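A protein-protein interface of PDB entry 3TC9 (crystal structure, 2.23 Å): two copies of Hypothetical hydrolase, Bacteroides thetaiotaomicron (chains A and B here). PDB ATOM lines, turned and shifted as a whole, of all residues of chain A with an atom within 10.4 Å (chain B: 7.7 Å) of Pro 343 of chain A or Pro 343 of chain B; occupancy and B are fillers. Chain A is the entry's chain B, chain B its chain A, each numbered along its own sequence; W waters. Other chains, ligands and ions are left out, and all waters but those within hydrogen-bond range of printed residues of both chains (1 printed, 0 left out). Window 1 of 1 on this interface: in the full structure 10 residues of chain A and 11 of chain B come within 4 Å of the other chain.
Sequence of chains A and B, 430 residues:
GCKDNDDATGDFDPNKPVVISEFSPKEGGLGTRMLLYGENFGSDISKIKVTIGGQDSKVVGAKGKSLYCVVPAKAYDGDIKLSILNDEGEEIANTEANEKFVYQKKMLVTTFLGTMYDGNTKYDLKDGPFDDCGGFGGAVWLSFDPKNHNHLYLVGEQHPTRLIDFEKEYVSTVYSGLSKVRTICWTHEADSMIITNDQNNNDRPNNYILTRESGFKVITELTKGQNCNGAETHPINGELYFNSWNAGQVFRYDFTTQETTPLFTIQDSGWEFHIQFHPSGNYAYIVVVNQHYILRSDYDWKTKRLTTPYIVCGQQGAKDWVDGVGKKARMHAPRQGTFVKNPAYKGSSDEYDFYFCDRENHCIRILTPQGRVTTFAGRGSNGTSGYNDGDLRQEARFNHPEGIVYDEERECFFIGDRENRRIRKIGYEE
Water W1 lies within hydrogen-bond range of the backbone carbonyl oxygen of Gly 347 of chain B and the side-chain amino group of Lys 105 of chain A.
Gly 347 of chain B touches Gln 104 of chain A. Pro 343 of chain B touches Pro 343 of chain A (CB to CB, 3.9 Å). Tyr 428 of chain B touches Lys 346 of chain A (CE2 to CG, 3.4 Å). Gly 347 of chain A touches Tyr 428 of chain B (CA to CE1, 3.9 Å). CG of Lys 346 of chain B touches OH of Tyr 428 of chain A, 3.6 Å away.
OE2 of Glu 351 of chain A sits at hydrogen-bond distance from N of Gly 347 of chain A (3.2 Å). The backbone NH (N) of Gly 347 of chain B lies within hydrogen-bond range of the side-chain carboxylate (OE2) of Glu 351 of chain B (3.2 Å).
Printed residues of chain B that touch a printed residue of chain A: Pro 343, Lys 346, Gly 347 and Tyr 428. Hydrophobic or aromatic side chains of chain B within 4 Å of the printed part of chain A: Pro 343 and Tyr 428. Of the 21 printed residues of chain A, 7 touch a printed residue of chain B. Among the printed residues, 8 pairs touch across the chains. Among the printed residues, Asp or Glu carboxylates within 4 Å of a Lys or Arg side-chain nitrogen of the other chain: Glu 411 of chain A with Lys 346 of chain B (3.4 Å).
Pro 343 of chain A touches its own counterpart, Pro 343 of chain B. Lys 346 of chain A touches Tyr 428 of chain B, and with the chains exchanged Tyr 428 of chain A touches Lys 346 of chain B. Gly 347 of chain A touches Tyr 428 of chain B, but with the chains exchanged Tyr 428 of chain A does not touch Gly 347 of chain B (4.4 Å). Positions printed for both chains: 340, 341, 342, 343, 344, 345, 346, 347, 351, 352, 353 and 428. Of the 8 pairs that touch across the chains among the printed residues, 3 have their exchanged pair printed and touching as well.
Pro 343 of chain A touches one residue of chain B. Printed residues of chain B within 4 Å of Glu 411 of chain A: Lys 346. Val 340 of chain B touches none of the printed residues of chain A. Of chain A, only Pro 343 (3.9 Å) comes within 4 Å of Pro 343 of chain B. Printed residues of chain A within 4 Å of Lys 346 of chain B: Gln 104, Glu 411 and Tyr 428. Of the printed residues of chain A, Gly 347 of chain B touches Gln 104 (3.6 Å) and Lys 105 (3.1 Å). Asp 353 of chain B touches none of the printed residues of chain A. Of the printed residues of chain A, Tyr 428 of chain B touches Lys 346 (3.4 Å) and Gly 347 (3.9 Å). The nearest residue of chain B that does not touch Pro 343 of chain A is Tyr 428 of chain B (6.1 Å). The nearest residue of chain A that does not touch Pro 343 of chain B is Tyr 428 of chain A (6.3 Å).
NZ of Lys 346 of chain B lies within salt-bridge range of OE2 of Glu 411 of chain A (3.4 Å). The backbone carbonyl oxygen (O) of Lys 346 of chain B sits at hydrogen-bond distance from the side-chain amide nitrogen (NE2) of Gln 104 of chain A (3.0 Å). N of Lys 105 of chain A lies within hydrogen-bond range of O of Gly 347 of chain B.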
ATOM      1  N   GLN A 104     -32.428   8.387 -10.733  1.00  0.00           N
ATOM      2  CA  GLN A 104     -32.079   8.801 -12.072  1.00  0.00           C
ATOM      3  C   GLN A 104     -31.238  10.079 -11.949  1.00  0.00           C
ATOM      4  O   GLN A 104     -31.753  11.103 -11.492  1.00  0.00           O
ATOM      5  CB  GLN A 104     -33.368   9.007 -12.920  1.00  0.00           C
ATOM      6  CG  GLN A 104     -33.175   9.718 -14.283  1.00  0.00           C
ATOM      7  CD  GLN A 104     -32.411   8.944 -15.340  1.00  0.00           C
ATOM      8  OE1 GLN A 104     -32.728   7.788 -15.671  1.00  0.00           O
ATOM      9  NE2 GLN A 104     -31.400   9.580 -15.922  1.00  0.00           N
ATOM     10  N   LYS A 105     -29.944  10.006 -12.321  1.00  0.00           N
ATOM     11  CA  LYS A 105     -29.050  11.157 -12.305  1.00  0.00           C
ATOM     12  C   LYS A 105     -29.427  12.188 -13.401  1.00  0.00           C
ATOM     13  O   LYS A 105     -29.933  11.840 -14.480  1.00  0.00           O
ATOM     14  CB  LYS A 105     -27.590  10.740 -12.533  1.00  0.00           C
ATOM     15  CG  LYS A 105     -26.930   9.909 -11.461  1.00  0.00           C
ATOM     16  CD  LYS A 105     -25.526   9.505 -11.937  1.00  0.00           C
ATOM     17  CE  LYS A 105     -24.743   8.657 -10.959  1.00  0.00           C
ATOM     18  NZ  LYS A 105     -25.306   7.283 -10.854  1.00  0.00           N
ATOM     19  N   VAL A 340     -21.811  19.357 -30.802  1.00  0.00           N
ATOM     20  CA  VAL A 340     -22.002  18.229 -29.891  1.00  0.00           C
ATOM     21  C   VAL A 340     -22.773  17.107 -30.618  1.00  0.00           C
ATOM     22  O   VAL A 340     -23.884  17.339 -31.125  1.00  0.00           O
ATOM     23  CB  VAL A 340     -22.742  18.688 -28.600  1.00  0.00           C
ATOM     24  CG1 VAL A 340     -22.941  17.521 -27.630  1.00  0.00           C
ATOM     25  CG2 VAL A 340     -21.998  19.840 -27.912  1.00  0.00           C
ATOM     26  N   LYS A 341     -22.187  15.899 -30.646  1.00  0.00           N
ATOM     27  CA  LYS A 341     -22.803  14.734 -31.285  1.00  0.00           C
ATOM     28  C   LYS A 341     -24.036  14.305 -30.509  1.00  0.00           C
ATOM     29  O   LYS A 341     -23.955  14.043 -29.310  1.00  0.00           O
ATOM     30  CB  LYS A 341     -21.806  13.582 -31.409  1.00  0.00           C
ATOM     31  CG  LYS A 341     -22.162  12.585 -32.501  1.00  0.00           C
ATOM     32  CD  LYS A 341     -21.038  11.572 -32.711  1.00  0.00           C
ATOM     33  CE  LYS A 341     -20.972  11.105 -34.135  1.00  0.00           C
ATOM     34  NZ  LYS A 341     -19.664  10.466 -34.437  1.00  0.00           N
ATOM     35  N   ASN A 342     -25.185  14.317 -31.182  1.00  0.00           N
ATOM     36  CA  ASN A 342     -26.460  13.925 -30.604  1.00  0.00           C
ATOM     37  C   ASN A 342     -26.794  12.457 -31.011  1.00  0.00           C
ATOM     38  O   ASN A 342     -27.023  12.190 -32.180  1.00  0.00           O
ATOM     39  CB  ASN A 342     -27.555  14.885 -31.028  1.00  0.00           C
ATOM     40  CG  ASN A 342     -28.896  14.668 -30.365  1.00  0.00           C
ATOM     41  OD1 ASN A 342     -29.287  13.564 -30.006  1.00  0.00           O
ATOM     42  ND2 ASN A 342     -29.668  15.719 -30.243  1.00  0.00           N
ATOM     43  N   PRO A 343     -26.864  11.517 -30.024  1.00  0.00           N
ATOM     44  CA  PRO A 343     -27.185  10.107 -30.337  1.00  0.00           C
ATOM     45  C   PRO A 343     -28.539   9.905 -31.031  1.00  0.00           C
ATOM     46  O   PRO A 343     -28.720   8.899 -31.734  1.00  0.00           O
ATOM     47  CB  PRO A 343     -27.194   9.445 -28.954  1.00  0.00           C
ATOM     48  CG  PRO A 343     -26.303  10.309 -28.120  1.00  0.00           C
ATOM     49  CD  PRO A 343     -26.628  11.696 -28.574  1.00  0.00           C
ATOM     50  N   ALA A 344     -29.481  10.873 -30.874  1.00  0.00           N
ATOM     51  CA  ALA A 344     -30.793  10.831 -31.530  1.00  0.00           C
ATOM     52  C   ALA A 344     -30.673  11.062 -33.050  1.00  0.00           C
ATOM     53  O   ALA A 344     -31.615  10.768 -33.775  1.00  0.00           O
ATOM     54  CB  ALA A 344     -31.714  11.873 -30.910  1.00  0.00           C
ATOM     55  N   TYR A 345     -29.536  11.606 -33.527  1.00  0.00           N
ATOM     56  CA  TYR A 345     -29.354  11.890 -34.958  1.00  0.00           C
ATOM     57  C   TYR A 345     -28.524  10.823 -35.669  1.00  0.00           C
ATOM     58  O   TYR A 345     -28.099  11.062 -36.802  1.00  0.00           O
ATOM     59  CB  TYR A 345     -28.663  13.253 -35.182  1.00  0.00           C
ATOM     60  CG  TYR A 345     -29.277  14.488 -34.565  1.00  0.00           C
ATOM     61  CD1 TYR A 345     -30.613  14.505 -34.159  1.00  0.00           C
ATOM     62  CD2 TYR A 345     -28.572  15.683 -34.520  1.00  0.00           C
ATOM     63  CE1 TYR A 345     -31.185  15.646 -33.595  1.00  0.00           C
ATOM     64  CE2 TYR A 345     -29.136  16.837 -33.985  1.00  0.00           C
ATOM     65  CZ  TYR A 345     -30.444  16.817 -33.515  1.00  0.00           C
ATOM     66  OH  TYR A 345     -31.013  17.962 -32.988  1.00  0.00           O
ATOM     67  N   LYS A 346     -28.238   9.683 -35.006  1.00  0.00           N
ATOM     68  CA  LYS A 346     -27.438   8.603 -35.595  1.00  0.00           C
ATOM     69  C   LYS A 346     -28.009   8.197 -36.981  1.00  0.00           C
ATOM     70  O   LYS A 346     -29.211   7.991 -37.122  1.00  0.00           O
ATOM     71  CB  LYS A 346     -27.349   7.397 -34.635  1.00  0.00           C
ATOM     72  CG  LYS A 346     -26.346   6.308 -35.022  1.00  0.00           C
ATOM     73  CD  LYS A 346     -24.868   6.682 -34.952  1.00  0.00           C
ATOM     74  CE  LYS A 346     -24.000   5.586 -35.560  1.00  0.00           C
ATOM     75  NZ  LYS A 346     -22.625   6.065 -35.873  1.00  0.00           N
ATOM     76  N   GLY A 347     -27.133   8.179 -37.983  1.00  0.00           N
ATOM     77  CA  GLY A 347     -27.492   7.833 -39.351  1.00  0.00           C
ATOM     78  C   GLY A 347     -27.837   9.035 -40.219  1.00  0.00           C
ATOM     79  O   GLY A 347     -27.777   8.955 -41.452  1.00  0.00           O
ATOM     80  N   SER A 348     -28.167  10.185 -39.601  1.00  0.00           N
ATOM     81  CA  SER A 348     -28.531  11.347 -40.405  1.00  0.00           C
ATOM     82  C   SER A 348     -27.294  12.061 -40.980  1.00  0.00           C
ATOM     83  O   SER A 348     -26.165  11.793 -40.567  1.00  0.00           O
ATOM     84  CB  SER A 348     -29.403  12.308 -39.612  1.00  0.00           C
ATOM     85  OG  SER A 348     -28.696  12.933 -38.568  1.00  0.00           O
ATOM     86  N   ASP A 350     -26.469  15.276 -40.688  1.00  0.00           N
ATOM     87  CA  ASP A 350     -25.871  16.050 -39.608  1.00  0.00           C
ATOM     88  C   ASP A 350     -26.172  15.400 -38.241  1.00  0.00           C
ATOM     89  O   ASP A 350     -27.310  15.407 -37.794  1.00  0.00           O
ATOM     90  CB  ASP A 350     -26.385  17.486 -39.649  1.00  0.00           C
ATOM     91  CG  ASP A 350     -25.472  18.504 -38.974  1.00  0.00           C
ATOM     92  OD1 ASP A 350     -24.739  18.119 -38.034  1.00  0.00           O
ATOM     93  OD2 ASP A 350     -25.490  19.682 -39.389  1.00  0.00           O
ATOM     94  N   GLU A 351     -25.148  14.868 -37.575  1.00  0.00           N
ATOM     95  CA  GLU A 351     -25.286  14.182 -36.305  1.00  0.00           C
ATOM     96  C   GLU A 351     -25.017  15.086 -35.110  1.00  0.00           C
ATOM     97  O   GLU A 351     -25.014  14.621 -33.966  1.00  0.00           O
ATOM     98  CB  GLU A 351     -24.336  12.972 -36.269  1.00  0.00           C
ATOM     99  CG  GLU A 351     -24.745  11.827 -37.189  1.00  0.00           C
ATOM    100  CD  GLU A 351     -24.164  10.463 -36.863  1.00  0.00           C
ATOM    101  OE1 GLU A 351     -23.696  10.265 -35.718  1.00  0.00           O
ATOM    102  OE2 GLU A 351     -24.234   9.566 -37.736  1.00  0.00           O
ATOM    103  N   TYR A 352     -24.766  16.358 -35.361  1.00  0.00           N
ATOM    104  CA  TYR A 352     -24.416  17.274 -34.290  1.00  0.00           C
ATOM    105  C   TYR A 352     -25.408  18.384 -34.102  1.00  0.00           C
ATOM    106  O   TYR A 352     -26.036  18.808 -35.050  1.00  0.00           O
ATOM    107  CB  TYR A 352     -23.037  17.923 -34.546  1.00  0.00           C
ATOM    108  CG  TYR A 352     -21.894  16.949 -34.683  1.00  0.00           C
ATOM    109  CD1 TYR A 352     -21.682  16.248 -35.873  1.00  0.00           C
ATOM    110  CD2 TYR A 352     -20.986  16.764 -33.649  1.00  0.00           C
ATOM    111  CE1 TYR A 352     -20.617  15.366 -36.013  1.00  0.00           C
ATOM    112  CE2 TYR A 352     -19.928  15.865 -33.768  1.00  0.00           C
ATOM    113  CZ  TYR A 352     -19.745  15.169 -34.952  1.00  0.00           C
ATOM    114  OH  TYR A 352     -18.689  14.299 -35.070  1.00  0.00           O
ATOM    115  N   ASP A 353     -25.488  18.876 -32.867  1.00  0.00           N
ATOM    116  CA  ASP A 353     -26.176  20.088 -32.449  1.00  0.00           C
ATOM    117  C   ASP A 353     -25.083  21.147 -32.210  1.00  0.00           C
ATOM    118  O   ASP A 353     -23.913  20.818 -31.936  1.00  0.00           O
ATOM    119  CB  ASP A 353     -26.975  19.853 -31.160  1.00  0.00           C
ATOM    120  CG  ASP A 353     -28.278  19.108 -31.292  1.00  0.00           C
ATOM    121  OD1 ASP A 353     -29.046  19.429 -32.205  1.00  0.00           O
ATOM    122  OD2 ASP A 353     -28.579  18.296 -30.411  1.00  0.00           O
ATOM    123  N   TYR A 355     -24.159  24.119 -29.699  1.00  0.00           N
ATOM    124  CA  TYR A 355     -24.330  24.747 -28.390  1.00  0.00           C
ATOM    125  C   TYR A 355     -23.518  26.018 -28.337  1.00  0.00           C
ATOM    126  O   TYR A 355     -22.329  25.972 -28.599  1.00  0.00           O
ATOM    127  CB  TYR A 355     -23.849  23.806 -27.283  1.00  0.00           C
ATOM    128  CG  TYR A 355     -24.789  22.666 -26.967  1.00  0.00           C
ATOM    129  CD1 TYR A 355     -25.002  21.640 -27.882  1.00  0.00           C
ATOM    130  CD2 TYR A 355     -25.392  22.559 -25.714  1.00  0.00           C
ATOM    131  CE1 TYR A 355     -25.809  20.546 -27.574  1.00  0.00           C
ATOM    132  CE2 TYR A 355     -26.197  21.466 -25.393  1.00  0.00           C
ATOM    133  CZ  TYR A 355     -26.407  20.465 -26.333  1.00  0.00           C
ATOM    134  OH  TYR A 355     -27.217  19.395 -26.061  1.00  0.00           O
ATOM    135  N   TYR A 406     -17.183  21.473 -25.671  1.00  0.00           N
ATOM    136  CA  TYR A 406     -17.725  20.210 -25.207  1.00  0.00           C
ATOM    137  C   TYR A 406     -16.548  19.204 -25.122  1.00  0.00           C
ATOM    138  O   TYR A 406     -15.742  19.105 -26.055  1.00  0.00           O
ATOM    139  CB  TYR A 406     -18.878  19.698 -26.092  1.00  0.00           C
ATOM    140  CG  TYR A 406     -19.455  18.380 -25.604  1.00  0.00           C
ATOM    141  CD1 TYR A 406     -20.121  18.296 -24.385  1.00  0.00           C
ATOM    142  CD2 TYR A 406     -19.294  17.208 -26.341  1.00  0.00           C
ATOM    143  CE1 TYR A 406     -20.582  17.074 -23.891  1.00  0.00           C
ATOM    144  CE2 TYR A 406     -19.748  15.977 -25.852  1.00  0.00           C
ATOM    145  CZ  TYR A 406     -20.399  15.920 -24.632  1.00  0.00           C
ATOM    146  OH  TYR A 406     -20.858  14.731 -24.140  1.00  0.00           O
ATOM    147  N   GLU A 408     -15.804  15.471 -25.113  1.00  0.00           N
ATOM    148  CA  GLU A 408     -16.376  14.154 -25.432  1.00  0.00           C
ATOM    149  C   GLU A 408     -15.865  13.043 -24.505  1.00  0.00           C
ATOM    150  O   GLU A 408     -16.634  12.168 -24.147  1.00  0.00           O
ATOM    151  CB  GLU A 408     -16.107  13.777 -26.897  1.00  0.00           C
ATOM    152  CG  GLU A 408     -16.898  14.633 -27.871  1.00  0.00           C
ATOM    153  CD  GLU A 408     -16.811  14.256 -29.339  1.00  0.00           C
ATOM    154  OE1 GLU A 408     -17.522  13.314 -29.764  1.00  0.00           O
ATOM    155  OE2 GLU A 408     -16.100  14.970 -30.082  1.00  0.00           O
ATOM    156  N   GLU A 411     -17.203  13.924 -20.963  1.00  0.00           N
ATOM    157  CA  GLU A 411     -18.675  14.021 -21.132  1.00  0.00           C
ATOM    158  C   GLU A 411     -19.273  15.250 -20.415  1.00  0.00           C
ATOM    159  O   GLU A 411     -20.267  15.149 -19.696  1.00  0.00           O
ATOM    160  CB  GLU A 411     -19.368  12.727 -20.686  1.00  0.00           C
ATOM    161  CG  GLU A 411     -18.984  11.519 -21.528  1.00  0.00           C
ATOM    162  CD  GLU A 411     -19.314  10.186 -20.892  1.00  0.00           C
ATOM    163  OE1 GLU A 411     -18.600   9.783 -19.943  1.00  0.00           O
ATOM    164  OE2 GLU A 411     -20.288   9.542 -21.344  1.00  0.00           O
ATOM    165  N   PHE A 413     -19.358  19.988 -20.502  1.00  0.00           N
ATOM    166  CA  PHE A 413     -19.088  21.304 -21.060  1.00  0.00           C
ATOM    167  C   PHE A 413     -18.247  22.100 -20.095  1.00  0.00           C
ATOM    168  O   PHE A 413     -18.442  21.998 -18.888  1.00  0.00           O
ATOM    169  CB  PHE A 413     -20.395  22.090 -21.335  1.00  0.00           C
ATOM    170  CG  PHE A 413     -21.329  21.478 -22.350  1.00  0.00           C
ATOM    171  CD1 PHE A 413     -22.235  20.480 -21.977  1.00  0.00           C
ATOM    172  CD2 PHE A 413     -21.308  21.897 -23.685  1.00  0.00           C
ATOM    173  CE1 PHE A 413     -23.088  19.902 -22.919  1.00  0.00           C
ATOM    174  CE2 PHE A 413     -22.176  21.333 -24.621  1.00  0.00           C
ATOM    175  CZ  PHE A 413     -23.051  20.329 -24.234  1.00  0.00           C
ATOM    176  N   TYR A 428     -23.243  15.413 -15.803  1.00  0.00           N
ATOM    177  CA  TYR A 428     -24.085  14.614 -14.897  1.00  0.00           C
ATOM    178  C   TYR A 428     -23.543  14.615 -13.470  1.00  0.00           C
ATOM    179  O   TYR A 428     -22.325  14.741 -13.272  1.00  0.00           O
ATOM    180  CB  TYR A 428     -24.143  13.154 -15.380  1.00  0.00           C
ATOM    181  CG  TYR A 428     -25.154  12.949 -16.479  1.00  0.00           C
ATOM    182  CD1 TYR A 428     -26.492  12.702 -16.184  1.00  0.00           C
ATOM    183  CD2 TYR A 428     -24.791  13.065 -17.816  1.00  0.00           C
ATOM    184  CE1 TYR A 428     -27.446  12.588 -17.190  1.00  0.00           C
ATOM    185  CE2 TYR A 428     -25.736  12.937 -18.833  1.00  0.00           C
ATOM    186  CZ  TYR A 428     -27.065  12.702 -18.513  1.00  0.00           C
ATOM    187  OH  TYR A 428     -28.008  12.554 -19.495  1.00  0.00           O
ATOM    188  N   VAL B 340     -26.238  -4.345 -24.407  1.00  0.00           N
ATOM    189  CA  VAL B 340     -26.012  -3.198 -25.298  1.00  0.00           C
ATOM    190  C   VAL B 340     -26.375  -1.903 -24.579  1.00  0.00           C
ATOM    191  O   VAL B 340     -27.507  -1.751 -24.108  1.00  0.00           O
ATOM    192  CB  VAL B 340     -26.815  -3.362 -26.630  1.00  0.00           C
ATOM    193  CG1 VAL B 340     -26.606  -2.164 -27.563  1.00  0.00           C
ATOM    194  CG2 VAL B 340     -26.469  -4.686 -27.336  1.00  0.00           C
ATOM    195  N   LYS B 341     -25.411  -0.976 -24.485  1.00  0.00           N
ATOM    196  CA  LYS B 341     -25.592   0.323 -23.836  1.00  0.00           C
ATOM    197  C   LYS B 341     -26.571   1.165 -24.639  1.00  0.00           C
ATOM    198  O   LYS B 341     -26.358   1.422 -25.831  1.00  0.00           O
ATOM    199  CB  LYS B 341     -24.255   1.059 -23.655  1.00  0.00           C
ATOM    200  CG  LYS B 341     -24.294   2.139 -22.573  1.00  0.00           C
ATOM    201  CD  LYS B 341     -22.899   2.678 -22.269  1.00  0.00           C
ATOM    202  CE  LYS B 341     -22.722   3.048 -20.816  1.00  0.00           C
ATOM    203  NZ  LYS B 341     -21.292   3.083 -20.426  1.00  0.00           N
ATOM    204  N   ASN B 342     -27.667   1.535 -23.986  1.00  0.00           N
ATOM    205  CA  ASN B 342     -28.725   2.335 -24.570  1.00  0.00           C
ATOM    206  C   ASN B 342     -28.559   3.816 -24.148  1.00  0.00           C
ATOM    207  O   ASN B 342     -28.718   4.128 -22.961  1.00  0.00           O
ATOM    208  CB  ASN B 342     -30.091   1.779 -24.174  1.00  0.00           C
ATOM    209  CG  ASN B 342     -31.255   2.427 -24.870  1.00  0.00           C
ATOM    210  OD1 ASN B 342     -31.238   3.608 -25.214  1.00  0.00           O
ATOM    211  ND2 ASN B 342     -32.314   1.676 -25.055  1.00  0.00           N
ATOM    212  N   PRO B 343     -28.294   4.737 -25.128  1.00  0.00           N
ATOM    213  CA  PRO B 343     -28.151   6.171 -24.799  1.00  0.00           C
ATOM    214  C   PRO B 343     -29.393   6.788 -24.132  1.00  0.00           C
ATOM    215  O   PRO B 343     -29.260   7.791 -23.430  1.00  0.00           O
ATOM    216  CB  PRO B 343     -27.895   6.824 -26.169  1.00  0.00           C
ATOM    217  CG  PRO B 343     -27.361   5.727 -27.027  1.00  0.00           C
ATOM    218  CD  PRO B 343     -28.112   4.509 -26.583  1.00  0.00           C
ATOM    219  N   ALA B 344     -30.587   6.190 -24.331  1.00  0.00           N
ATOM    220  CA  ALA B 344     -31.825   6.660 -23.713  1.00  0.00           C
ATOM    221  C   ALA B 344     -31.844   6.387 -22.194  1.00  0.00           C
ATOM    222  O   ALA B 344     -32.676   6.959 -21.491  1.00  0.00           O
ATOM    223  CB  ALA B 344     -33.028   5.999 -24.372  1.00  0.00           C
ATOM    224  N   TYR B 345     -30.965   5.491 -21.692  1.00  0.00           N
ATOM    225  CA  TYR B 345     -30.926   5.153 -20.276  1.00  0.00           C
ATOM    226  C   TYR B 345     -29.814   5.888 -19.537  1.00  0.00           C
ATOM    227  O   TYR B 345     -29.541   5.526 -18.397  1.00  0.00           O
ATOM    228  CB  TYR B 345     -30.733   3.640 -20.051  1.00  0.00           C
ATOM    229  CG  TYR B 345     -31.703   2.674 -20.712  1.00  0.00           C
ATOM    230  CD1 TYR B 345     -32.953   3.100 -21.159  1.00  0.00           C
ATOM    231  CD2 TYR B 345     -31.433   1.309 -20.749  1.00  0.00           C
ATOM    232  CE1 TYR B 345     -33.851   2.210 -21.749  1.00  0.00           C
ATOM    233  CE2 TYR B 345     -32.339   0.404 -21.305  1.00  0.00           C
ATOM    234  CZ  TYR B 345     -33.545   0.859 -21.806  1.00  0.00           C
ATOM    235  OH  TYR B 345     -34.419  -0.029 -22.372  1.00  0.00           O
ATOM    236  N   LYS B 346     -29.147   6.876 -20.173  1.00  0.00           N
ATOM    237  CA  LYS B 346     -28.045   7.635 -19.562  1.00  0.00           C
ATOM    238  C   LYS B 346     -28.477   8.213 -18.212  1.00  0.00           C
ATOM    239  O   LYS B 346     -29.550   8.802 -18.110  1.00  0.00           O
ATOM    240  CB  LYS B 346     -27.535   8.739 -20.509  1.00  0.00           C
ATOM    241  CG  LYS B 346     -26.231   9.434 -20.084  1.00  0.00           C
ATOM    242  CD  LYS B 346     -24.974   8.549 -20.169  1.00  0.00           C
ATOM    243  CE  LYS B 346     -23.759   9.267 -19.643  1.00  0.00           C
ATOM    244  NZ  LYS B 346     -22.658   8.329 -19.296  1.00  0.00           N
ATOM    245  N   GLY B 347     -27.687   7.940 -17.187  1.00  0.00           N
ATOM    246  CA  GLY B 347     -27.978   8.406 -15.832  1.00  0.00           C
ATOM    247  C   GLY B 347     -28.729   7.413 -14.973  1.00  0.00           C
ATOM    248  O   GLY B 347     -28.735   7.542 -13.758  1.00  0.00           O
ATOM    249  N   GLU B 351     -28.036   0.940 -17.588  1.00  0.00           N
ATOM    250  CA  GLU B 351     -27.900   1.640 -18.861  1.00  0.00           C
ATOM    251  C   GLU B 351     -27.904   0.687 -20.070  1.00  0.00           C
ATOM    252  O   GLU B 351     -27.696   1.133 -21.189  1.00  0.00           O
ATOM    253  CB  GLU B 351     -26.611   2.481 -18.854  1.00  0.00           C
ATOM    254  CG  GLU B 351     -26.652   3.697 -17.926  1.00  0.00           C
ATOM    255  CD  GLU B 351     -25.623   4.784 -18.216  1.00  0.00           C
ATOM    256  OE1 GLU B 351     -25.067   4.788 -19.337  1.00  0.00           O
ATOM    257  OE2 GLU B 351     -25.406   5.663 -17.341  1.00  0.00           O
ATOM    258  N   TYR B 352     -28.189  -0.604 -19.851  1.00  0.00           N
ATOM    259  CA  TYR B 352     -28.114  -1.637 -20.884  1.00  0.00           C
ATOM    260  C   TYR B 352     -29.403  -2.387 -21.162  1.00  0.00           C
ATOM    261  O   TYR B 352     -30.165  -2.715 -20.256  1.00  0.00           O
ATOM    262  CB  TYR B 352     -27.062  -2.697 -20.484  1.00  0.00           C
ATOM    263  CG  TYR B 352     -25.655  -2.167 -20.363  1.00  0.00           C
ATOM    264  CD1 TYR B 352     -25.215  -1.541 -19.189  1.00  0.00           C
ATOM    265  CD2 TYR B 352     -24.742  -2.314 -21.405  1.00  0.00           C
ATOM    266  CE1 TYR B 352     -23.928  -0.998 -19.098  1.00  0.00           C
ATOM    267  CE2 TYR B 352     -23.425  -1.856 -21.289  1.00  0.00           C
ATOM    268  CZ  TYR B 352     -23.029  -1.188 -20.147  1.00  0.00           C
ATOM    269  OH  TYR B 352     -21.731  -0.755 -20.060  1.00  0.00           O
ATOM    270  N   ASP B 353     -29.587  -2.725 -22.436  1.00  0.00           N
ATOM    271  CA  ASP B 353     -30.627  -3.627 -22.937  1.00  0.00           C
ATOM    272  C   ASP B 353     -29.965  -4.993 -23.207  1.00  0.00           C
ATOM    273  O   ASP B 353     -28.745  -5.067 -23.429  1.00  0.00           O
ATOM    274  CB  ASP B 353     -31.259  -3.105 -24.237  1.00  0.00           C
ATOM    275  CG  ASP B 353     -32.222  -1.960 -24.091  1.00  0.00           C
ATOM    276  OD1 ASP B 353     -33.070  -2.019 -23.183  1.00  0.00           O
ATOM    277  OD2 ASP B 353     -32.208  -1.062 -24.967  1.00  0.00           O
ATOM    278  N   TYR B 428     -25.667   0.308 -39.336  1.00  0.00           N
ATOM    279  CA  TYR B 428     -26.086   1.372 -40.242  1.00  0.00           C
ATOM    280  C   TYR B 428     -25.433   1.176 -41.596  1.00  0.00           C
ATOM    281  O   TYR B 428     -24.289   0.710 -41.662  1.00  0.00           O
ATOM    282  CB  TYR B 428     -25.668   2.735 -39.654  1.00  0.00           C
ATOM    283  CG  TYR B 428     -26.657   3.254 -38.645  1.00  0.00           C
ATOM    284  CD1 TYR B 428     -27.786   3.964 -39.047  1.00  0.00           C
ATOM    285  CD2 TYR B 428     -26.502   2.987 -37.285  1.00  0.00           C
ATOM    286  CE1 TYR B 428     -28.746   4.383 -38.126  1.00  0.00           C
ATOM    287  CE2 TYR B 428     -27.464   3.388 -36.352  1.00  0.00           C
ATOM    288  CZ  TYR B 428     -28.572   4.107 -36.774  1.00  0.00           C
ATOM    289  OH  TYR B 428     -29.518   4.499 -35.854  1.00  0.00           O
HETATM  290  O   HOH W   1     -27.940   6.611 -11.339  1.00  0.00           O
